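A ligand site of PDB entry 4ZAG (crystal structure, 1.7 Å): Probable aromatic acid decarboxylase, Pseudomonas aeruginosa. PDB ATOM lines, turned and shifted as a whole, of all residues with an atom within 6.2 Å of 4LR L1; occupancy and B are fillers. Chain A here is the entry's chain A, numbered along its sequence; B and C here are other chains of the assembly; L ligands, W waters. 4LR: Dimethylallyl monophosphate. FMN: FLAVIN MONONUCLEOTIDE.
An oxygen (O4) of FMN L2 lies within hydrogen-bond range of the guanidinium group of Arg 139 of chain B. An oxygen (OAE) of 4LR L1 lies within salt-bridge range of the guanidinium group of Arg 122, 2.9 Å away. OAD of 4LR L1 is in hydrogen-bond range of N of Gly 91 (2.8 Å). OAD of 4LR L1 is in salt-bridge range of NH1 of Arg 185 of chain C, 2.7 Å away. O of Arg 139 of chain B sits at hydrogen-bond distance from N3 of FMN L2, at 3.1 Å. An oxygen (OAH) of 4LR L1 lies within hydrogen-bond range of the side-chain hydroxyl (OG) of Ser 90. O4 of FMN L2 is in hydrogen-bond range of N of Ser 15 of chain B (3.0 Å). OE1 of Glu 140 of chain B lies close to OAE of 4LR L1 (2.4 Å). An oxygen (OAD) of 4LR L1 lies within salt-bridge range of the side-chain amino group of Lys 129 (2.7 Å). An oxygen (OAC) of 4LR L1 is in salt-bridge range of the guanidinium group (NH2) of Arg 139 of chain B (3.2 Å). The side-chain hydroxyl of Tyr 169 of chain C is in hydrogen-bond range of an oxygen (OAC) of 4LR L1 (3.0 Å).
Merely in contact with 4LR L1: Trp 84 (3.4 Å), Ala 89 (3.5 Å) and Trp 200 of chain C (3.7 Å). Hydrophobic or aromatic side chains within 4 Å of 4LR L1: Ala 89, Tyr 169 of chain C and Trp 200 of chain C. Of the 21 residues printed, 11 come within 4 Å of 4LR L1. The nearest printed residue that does not touch 4LR L1 is Ser 92 (4.1 Å).
The backbone carbonyl oxygen (O) of Met 85 is in hydrogen-bond range of the indole nitrogen (NE1) of Trp 200 of chain C, at 3.5 Å. O of Ser 92 lies within hydrogen-bond range of N of Trp 200 of chain C. OG of Ser 92 lies within hydrogen-bond range of OG of Ser 90. O of Ala 86 lies close to NE1 of Trp 200 of chain C (3.5 Å). The indole nitrogen (NE1) of Trp 200 of chain C lies within hydrogen-bond range of the backbone carbonyl oxygen (O) of Trp 84 (2.9 Å). The side-chain carboxylate (OE2) of Glu 130 is in salt-bridge range of the side-chain amino group (NZ) of Lys 129 (2.7 Å). The side-chain carboxylate (OE2) of Glu 130 lies within salt-bridge range of the guanidinium group (NH1) of Arg 185 of chain C (3.0 Å). The guanidinium group of Arg 122 lies within salt-bridge range of the side-chain carboxylate of Glu 140 of chain B, 2.9 Å away.
Water W1 lies within hydrogen-bond range of NH1 of Arg 139 of chain B, OAC of 4LR L1, O of Ala 141 of chain B and NH2 of Arg 185 of chain C.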
ATOM      1  N   TRP A  84     -12.264  25.906   9.872  1.00  0.00           N
ATOM      2  CA  TRP A  84     -12.670  25.056   8.777  1.00  0.00           C
ATOM      3  C   TRP A  84     -14.093  24.526   8.926  1.00  0.00           C
ATOM      4  O   TRP A  84     -14.666  24.011   7.971  1.00  0.00           O
ATOM      5  CB  TRP A  84     -11.739  23.878   8.588  1.00  0.00           C
ATOM      6  CG  TRP A  84     -10.291  24.246   8.555  1.00  0.00           C
ATOM      7  CD1 TRP A  84      -9.345  23.875   9.491  1.00  0.00           C
ATOM      8  CD2 TRP A  84      -9.603  25.153   7.655  1.00  0.00           C
ATOM      9  NE1 TRP A  84      -8.141  24.480   9.224  1.00  0.00           N
ATOM     10  CE2 TRP A  84      -8.260  25.257   8.098  1.00  0.00           C
ATOM     11  CE3 TRP A  84     -10.008  25.909   6.523  1.00  0.00           C
ATOM     12  CZ2 TRP A  84      -7.302  26.074   7.463  1.00  0.00           C
ATOM     13  CZ3 TRP A  84      -9.020  26.693   5.861  1.00  0.00           C
ATOM     14  CH2 TRP A  84      -7.716  26.781   6.338  1.00  0.00           C
ATOM     15  N   MET A  85     -14.728  24.725  10.069  1.00  0.00           N
ATOM     16  CA  MET A  85     -16.156  24.416  10.198  1.00  0.00           C
ATOM     17  C   MET A  85     -17.065  25.440   9.544  1.00  0.00           C
ATOM     18  O   MET A  85     -18.261  25.206   9.474  1.00  0.00           O
ATOM     19  CB  MET A  85     -16.540  24.324  11.694  1.00  0.00           C
ATOM     20  CG  MET A  85     -16.119  23.038  12.384  1.00  0.00           C
ATOM     21  SD  MET A  85     -16.761  23.116  14.121  1.00  0.00           S
ATOM     22  CE  MET A  85     -16.271  21.472  14.717  1.00  0.00           C
ATOM     23  N   ALA A  86     -16.530  26.609   9.156  1.00  0.00           N
ATOM     24  CA  ALA A  86     -17.306  27.664   8.563  1.00  0.00           C
ATOM     25  C   ALA A  86     -17.710  27.265   7.162  1.00  0.00           C
ATOM     26  O   ALA A  86     -16.949  26.600   6.486  1.00  0.00           O
ATOM     27  CB  ALA A  86     -16.505  28.954   8.564  1.00  0.00           C
ATOM     28  N   ALA A  89     -15.367  27.160   3.838  1.00  0.00           N
ATOM     29  CA  ALA A  89     -14.334  26.137   3.680  1.00  0.00           C
ATOM     30  C   ALA A  89     -14.649  24.958   2.797  1.00  0.00           C
ATOM     31  O   ALA A  89     -13.698  24.210   2.360  1.00  0.00           O
ATOM     32  CB  ALA A  89     -13.878  25.640   5.052  1.00  0.00           C
ATOM     33  N   SER A  90     -15.919  24.773   2.480  1.00  0.00           N
ATOM     34  CA  SER A  90     -16.362  23.667   1.707  1.00  0.00           C
ATOM     35  C   SER A  90     -17.305  24.053   0.586  1.00  0.00           C
ATOM     36  O   SER A  90     -18.206  24.884   0.732  1.00  0.00           O
ATOM     37  CB  SER A  90     -17.108  22.631   2.588  1.00  0.00           C
ATOM     38  OG  SER A  90     -17.580  21.506   1.785  1.00  0.00           O
ATOM     39  N   GLY A  91     -17.133  23.383  -0.557  1.00  0.00           N
ATOM     40  CA  GLY A  91     -18.052  23.590  -1.631  1.00  0.00           C
ATOM     41  C   GLY A  91     -19.415  22.978  -1.402  1.00  0.00           C
ATOM     42  O   GLY A  91     -20.291  23.189  -2.231  1.00  0.00           O
ATOM     43  N   SER A  92     -19.583  22.187  -0.347  1.00  0.00           N
ATOM     44  CA  SER A  92     -20.880  21.635  -0.049  1.00  0.00           C
ATOM     45  C   SER A  92     -21.712  22.645   0.722  1.00  0.00           C
ATOM     46  O   SER A  92     -22.893  22.420   0.964  1.00  0.00           O
ATOM     47  CB  SER A  92     -20.733  20.302   0.716  1.00  0.00           C
ATOM     48  OG  SER A  92     -20.282  20.493   1.999  1.00  0.00           O
ATOM     49  N   ARG A 122      -8.663  29.513   1.359  1.00  0.00           N
ATOM     50  CA  ARG A 122      -9.480  28.385   1.062  1.00  0.00           C
ATOM     51  C   ARG A 122     -10.841  28.756   0.508  1.00  0.00           C
ATOM     52  O   ARG A 122     -11.357  28.095  -0.406  1.00  0.00           O
ATOM     53  CB  ARG A 122      -9.659  27.510   2.339  1.00  0.00           C
ATOM     54  CG  ARG A 122     -10.587  26.298   2.146  1.00  0.00           C
ATOM     55  CD  ARG A 122     -10.200  25.338   1.072  1.00  0.00           C
ATOM     56  NE  ARG A 122     -11.170  24.251   1.081  1.00  0.00           N
ATOM     57  CZ  ARG A 122     -11.228  23.293   0.180  1.00  0.00           C
ATOM     58  NH1 ARG A 122     -10.279  23.168  -0.772  1.00  0.00           N
ATOM     59  NH2 ARG A 122     -12.243  22.392   0.267  1.00  0.00           N
ATOM     60  N   VAL A 126     -12.424  27.510  -2.991  1.00  0.00           N
ATOM     61  CA  VAL A 126     -13.743  26.909  -3.119  1.00  0.00           C
ATOM     62  C   VAL A 126     -14.650  27.645  -4.103  1.00  0.00           C
ATOM     63  O   VAL A 126     -15.325  27.024  -4.918  1.00  0.00           O
ATOM     64  CB  VAL A 126     -14.408  26.822  -1.701  1.00  0.00           C
ATOM     65  CG1 VAL A 126     -15.888  26.480  -1.838  1.00  0.00           C
ATOM     66  CG2 VAL A 126     -13.665  25.853  -0.788  1.00  0.00           C
ATOM     67  N   LYS A 129     -13.559  26.653  -7.607  1.00  0.00           N
ATOM     68  CA  LYS A 129     -13.903  25.267  -7.991  1.00  0.00           C
ATOM     69  C   LYS A 129     -15.407  24.997  -8.172  1.00  0.00           C
ATOM     70  O   LYS A 129     -15.766  24.138  -8.982  1.00  0.00           O
ATOM     71  CB  LYS A 129     -13.238  24.278  -7.045  1.00  0.00           C
ATOM     72  CG  LYS A 129     -14.093  23.927  -5.801  1.00  0.00           C
ATOM     73  CD  LYS A 129     -13.214  23.153  -4.799  1.00  0.00           C
ATOM     74  CE  LYS A 129     -13.952  22.763  -3.498  1.00  0.00           C
ATOM     75  NZ  LYS A 129     -15.044  21.816  -3.729  1.00  0.00           N
ATOM     76  N   GLU A 130     -16.239  25.764  -7.427  1.00  0.00           N
ATOM     77  CA  GLU A 130     -17.642  25.735  -7.551  1.00  0.00           C
ATOM     78  C   GLU A 130     -18.222  26.656  -8.567  1.00  0.00           C
ATOM     79  O   GLU A 130     -19.443  26.653  -8.797  1.00  0.00           O
ATOM     80  CB  GLU A 130     -18.281  25.886  -6.175  1.00  0.00           C
ATOM     81  CG  GLU A 130     -17.899  24.902  -5.104  1.00  0.00           C
ATOM     82  CD  GLU A 130     -18.134  23.409  -5.377  1.00  0.00           C
ATOM     83  OE1 GLU A 130     -19.057  23.100  -6.165  1.00  0.00           O
ATOM     84  OE2 GLU A 130     -17.443  22.546  -4.817  1.00  0.00           O
ATOM     85  N   SER B  15     -10.038  15.480   3.008  1.00  0.00           N
ATOM     86  CA  SER B  15     -10.916  14.369   3.390  1.00  0.00           C
ATOM     87  C   SER B  15     -10.282  13.103   2.855  1.00  0.00           C
ATOM     88  O   SER B  15      -9.666  13.086   1.757  1.00  0.00           O
ATOM     89  CB  SER B  15     -12.329  14.612   2.909  1.00  0.00           C
ATOM     90  OG  SER B  15     -13.187  13.658   3.581  1.00  0.00           O
ATOM     91  N   ARG B 139      -7.726  14.677  -3.054  1.00  0.00           N
ATOM     92  CA  ARG B 139      -9.155  14.315  -2.813  1.00  0.00           C
ATOM     93  C   ARG B 139      -9.997  15.591  -2.799  1.00  0.00           C
ATOM     94  O   ARG B 139     -10.135  16.274  -1.800  1.00  0.00           O
ATOM     95  CB  ARG B 139      -9.297  13.580  -1.472  1.00  0.00           C
ATOM     96  CG  ARG B 139     -10.671  13.009  -1.158  1.00  0.00           C
ATOM     97  CD  ARG B 139     -11.670  14.054  -0.693  1.00  0.00           C
ATOM     98  NE  ARG B 139     -12.726  14.271  -1.684  1.00  0.00           N
ATOM     99  CZ  ARG B 139     -13.443  15.389  -1.735  1.00  0.00           C
ATOM    100  NH1 ARG B 139     -14.396  15.514  -2.621  1.00  0.00           N
ATOM    101  NH2 ARG B 139     -13.148  16.356  -0.879  1.00  0.00           N
ATOM    102  N   GLU B 140     -10.515  15.959  -3.954  1.00  0.00           N
ATOM    103  CA  GLU B 140     -11.251  17.210  -4.132  1.00  0.00           C
ATOM    104  C   GLU B 140     -12.215  16.950  -5.275  1.00  0.00           C
ATOM    105  O   GLU B 140     -12.019  16.116  -6.151  1.00  0.00           O
ATOM    106  CB  GLU B 140     -10.270  18.384  -4.462  1.00  0.00           C
ATOM    107  CG  GLU B 140     -10.926  19.801  -4.563  1.00  0.00           C
ATOM    108  CD  GLU B 140     -11.657  20.176  -3.325  1.00  0.00           C
ATOM    109  OE1 GLU B 140     -12.830  19.678  -3.171  1.00  0.00           O
ATOM    110  OE2 GLU B 140     -11.143  20.949  -2.497  1.00  0.00           O
ATOM    111  N   ALA B 141     -13.320  17.670  -5.252  1.00  0.00           N
ATOM    112  CA  ALA B 141     -14.265  17.694  -6.342  1.00  0.00           C
ATOM    113  C   ALA B 141     -15.164  18.939  -6.189  1.00  0.00           C
ATOM    114  O   ALA B 141     -15.612  19.238  -5.068  1.00  0.00           O
ATOM    115  CB  ALA B 141     -15.084  16.411  -6.419  1.00  0.00           C
ATOM    116  N   PRO B 142     -15.451  19.656  -7.264  1.00  0.00           N
ATOM    117  CA  PRO B 142     -14.739  19.550  -8.582  1.00  0.00           C
ATOM    118  C   PRO B 142     -13.269  19.879  -8.433  1.00  0.00           C
ATOM    119  O   PRO B 142     -12.879  20.473  -7.393  1.00  0.00           O
ATOM    120  CB  PRO B 142     -15.412  20.656  -9.440  1.00  0.00           C
ATOM    121  CG  PRO B 142     -16.695  20.912  -8.780  1.00  0.00           C
ATOM    122  CD  PRO B 142     -16.530  20.648  -7.314  1.00  0.00           C
ATOM    123  N   GLY C 167     -15.701  12.256  -0.613  1.00  0.00           N
ATOM    124  CA  GLY C 167     -15.281  12.706   0.687  1.00  0.00           C
ATOM    125  C   GLY C 167     -15.905  11.843   1.790  1.00  0.00           C
ATOM    126  O   GLY C 167     -16.790  11.023   1.549  1.00  0.00           O
ATOM    127  N   TYR C 169     -16.442  13.246   5.086  1.00  0.00           N
ATOM    128  CA  TYR C 169     -16.829  14.136   6.185  1.00  0.00           C
ATOM    129  C   TYR C 169     -18.312  14.014   6.623  1.00  0.00           C
ATOM    130  O   TYR C 169     -18.723  14.702   7.569  1.00  0.00           O
ATOM    131  CB  TYR C 169     -16.395  15.596   5.910  1.00  0.00           C
ATOM    132  CG  TYR C 169     -16.809  16.190   4.576  1.00  0.00           C
ATOM    133  CD1 TYR C 169     -18.070  16.776   4.392  1.00  0.00           C
ATOM    134  CD2 TYR C 169     -15.889  16.219   3.478  1.00  0.00           C
ATOM    135  CE1 TYR C 169     -18.415  17.368   3.198  1.00  0.00           C
ATOM    136  CE2 TYR C 169     -16.250  16.811   2.255  1.00  0.00           C
ATOM    137  CZ  TYR C 169     -17.496  17.398   2.135  1.00  0.00           C
ATOM    138  OH  TYR C 169     -17.867  17.993   0.975  1.00  0.00           O
ATOM    139  N   PHE C 181     -22.327  10.618  -2.217  1.00  0.00           N
ATOM    140  CA  PHE C 181     -21.514  11.827  -2.073  1.00  0.00           C
ATOM    141  C   PHE C 181     -21.198  12.435  -3.458  1.00  0.00           C
ATOM    142  O   PHE C 181     -21.445  13.613  -3.660  1.00  0.00           O
ATOM    143  CB  PHE C 181     -20.191  11.538  -1.327  1.00  0.00           C
ATOM    144  CG  PHE C 181     -19.361  12.777  -1.068  1.00  0.00           C
ATOM    145  CD1 PHE C 181     -18.595  13.321  -2.126  1.00  0.00           C
ATOM    146  CD2 PHE C 181     -19.307  13.405   0.169  1.00  0.00           C
ATOM    147  CE1 PHE C 181     -17.864  14.489  -1.960  1.00  0.00           C
ATOM    148  CE2 PHE C 181     -18.549  14.528   0.361  1.00  0.00           C
ATOM    149  CZ  PHE C 181     -17.862  15.095  -0.705  1.00  0.00           C
ATOM    150  N   ARG C 185     -22.663  16.008  -5.276  1.00  0.00           N
ATOM    151  CA  ARG C 185     -21.865  17.110  -5.770  1.00  0.00           C
ATOM    152  C   ARG C 185     -22.246  17.441  -7.192  1.00  0.00           C
ATOM    153  O   ARG C 185     -22.270  18.626  -7.538  1.00  0.00           O
ATOM    154  CB  ARG C 185     -20.366  16.788  -5.659  1.00  0.00           C
ATOM    155  CG  ARG C 185     -19.965  16.447  -4.248  1.00  0.00           C
ATOM    156  CD  ARG C 185     -20.235  17.584  -3.276  1.00  0.00           C
ATOM    157  NE  ARG C 185     -19.341  18.707  -3.496  1.00  0.00           N
ATOM    158  CZ  ARG C 185     -18.528  19.224  -2.575  1.00  0.00           C
ATOM    159  NH1 ARG C 185     -17.751  20.228  -2.870  1.00  0.00           N
ATOM    160  NH2 ARG C 185     -18.465  18.726  -1.381  1.00  0.00           N
ATOM    161  N   TRP C 200     -22.552  22.292   4.371  1.00  0.00           N
ATOM    162  CA  TRP C 200     -21.505  22.474   5.363  1.00  0.00           C
ATOM    163  C   TRP C 200     -21.612  23.752   6.167  1.00  0.00           C
ATOM    164  O   TRP C 200     -21.661  24.826   5.610  1.00  0.00           O
ATOM    165  CB  TRP C 200     -20.099  22.482   4.668  1.00  0.00           C
ATOM    166  CG  TRP C 200     -18.975  22.476   5.606  1.00  0.00           C
ATOM    167  CD1 TRP C 200     -18.149  23.532   5.900  1.00  0.00           C
ATOM    168  CD2 TRP C 200     -18.519  21.369   6.418  1.00  0.00           C
ATOM    169  NE1 TRP C 200     -17.220  23.148   6.842  1.00  0.00           N
ATOM    170  CE2 TRP C 200     -17.420  21.822   7.153  1.00  0.00           C
ATOM    171  CE3 TRP C 200     -18.949  20.025   6.567  1.00  0.00           C
ATOM    172  CZ2 TRP C 200     -16.744  21.001   8.070  1.00  0.00           C
ATOM    173  CZ3 TRP C 200     -18.279  19.218   7.443  1.00  0.00           C
ATOM    174  CH2 TRP C 200     -17.190  19.693   8.194  1.00  0.00           C
HETATM  175  OAD 4LR L   1     -15.795  21.084  -1.282  1.00  0.00           O
HETATM  176  PAJ 4LR L   1     -15.065  20.041  -0.477  1.00  0.00           P
HETATM  177  OAE 4LR L   1     -13.493  20.000  -0.849  1.00  0.00           O
HETATM  178  OAC 4LR L   1     -15.434  18.617  -0.583  1.00  0.00           O
HETATM  179  OAH 4LR L   1     -15.029  20.566   1.007  1.00  0.00           O
HETATM  180  CAG 4LR L   1     -14.247  19.751   1.967  1.00  0.00           C
HETATM  181  CAF 4LR L   1     -13.936  20.815   3.009  1.00  0.00           C
HETATM  182  CAI 4LR L   1     -14.574  20.842   4.320  1.00  0.00           C
HETATM  183  CAB 4LR L   1     -15.553  19.697   4.667  1.00  0.00           C
HETATM  184  CAA 4LR L   1     -14.123  21.871   5.374  1.00  0.00           C
HETATM  185  N1  FMN L   2      -9.170  20.481   1.522  1.00  0.00           N
HETATM  186  C2  FMN L   2      -9.123  19.780   0.360  1.00  0.00           C
HETATM  187  O2  FMN L   2      -8.348  20.216  -0.537  1.00  0.00           O
HETATM  188  N3  FMN L   2      -9.849  18.673   0.111  1.00  0.00           N
HETATM  189  C4  FMN L   2     -10.680  18.169   1.107  1.00  0.00           C
HETATM  190  O4  FMN L   2     -11.292  17.137   0.899  1.00  0.00           O
HETATM  191  C4A FMN L   2     -10.718  18.884   2.327  1.00  0.00           C
HETATM  192  N5  FMN L   2     -11.495  18.347   3.350  1.00  0.00           N
HETATM  193  C5A FMN L   2     -11.416  19.027   4.511  1.00  0.00           C
HETATM  194  C6  FMN L   2     -12.227  18.393   5.518  1.00  0.00           C
HETATM  195  C7  FMN L   2     -12.240  18.965   6.773  1.00  0.00           C
HETATM  196  C7M FMN L   2     -13.104  18.360   7.837  1.00  0.00           C
HETATM  197  C8  FMN L   2     -11.503  20.064   7.023  1.00  0.00           C
HETATM  198  C8M FMN L   2     -11.587  20.673   8.310  1.00  0.00           C
HETATM  199  C9  FMN L   2     -10.712  20.708   6.026  1.00  0.00           C
HETATM  200  C9A FMN L   2     -10.726  20.180   4.745  1.00  0.00           C
HETATM  201  N10 FMN L   2      -9.988  20.735   3.710  1.00  0.00           N
HETATM  202  C10 FMN L   2      -9.982  20.039   2.552  1.00  0.00           C
HETATM  203  C1' FMN L   2      -9.289  21.938   3.955  1.00  0.00           C
HETATM  204  C2' FMN L   2      -7.867  22.059   4.330  1.00  0.00           C
HETATM  205  O2' FMN L   2      -7.712  21.236   5.452  1.00  0.00           O
HETATM  206  C3' FMN L   2      -7.328  23.417   4.287  1.00  0.00           C
HETATM  207  O3' FMN L   2      -7.405  24.085   3.028  1.00  0.00           O
HETATM  208  C4' FMN L   2      -5.945  23.411   4.949  1.00  0.00           C
HETATM  209  O4' FMN L   2      -5.405  24.717   4.850  1.00  0.00           O
HETATM  210  C5' FMN L   2      -5.040  22.406   4.347  1.00  0.00           C
HETATM  211  O5' FMN L   2      -3.845  22.577   5.044  1.00  0.00           O
HETATM  212  P   FMN L   2      -2.713  21.471   4.846  1.00  0.00           P
HETATM  213  O1P FMN L   2      -1.454  22.035   5.581  1.00  0.00           O
HETATM  214  O2P FMN L   2      -3.106  20.102   5.425  1.00  0.00           O
HETATM  215  O3P FMN L   2      -2.496  21.351   3.301  1.00  0.00           O
HETATM  216  O   HOH W   1     -16.002  17.482  -2.971  1.00  0.00           O
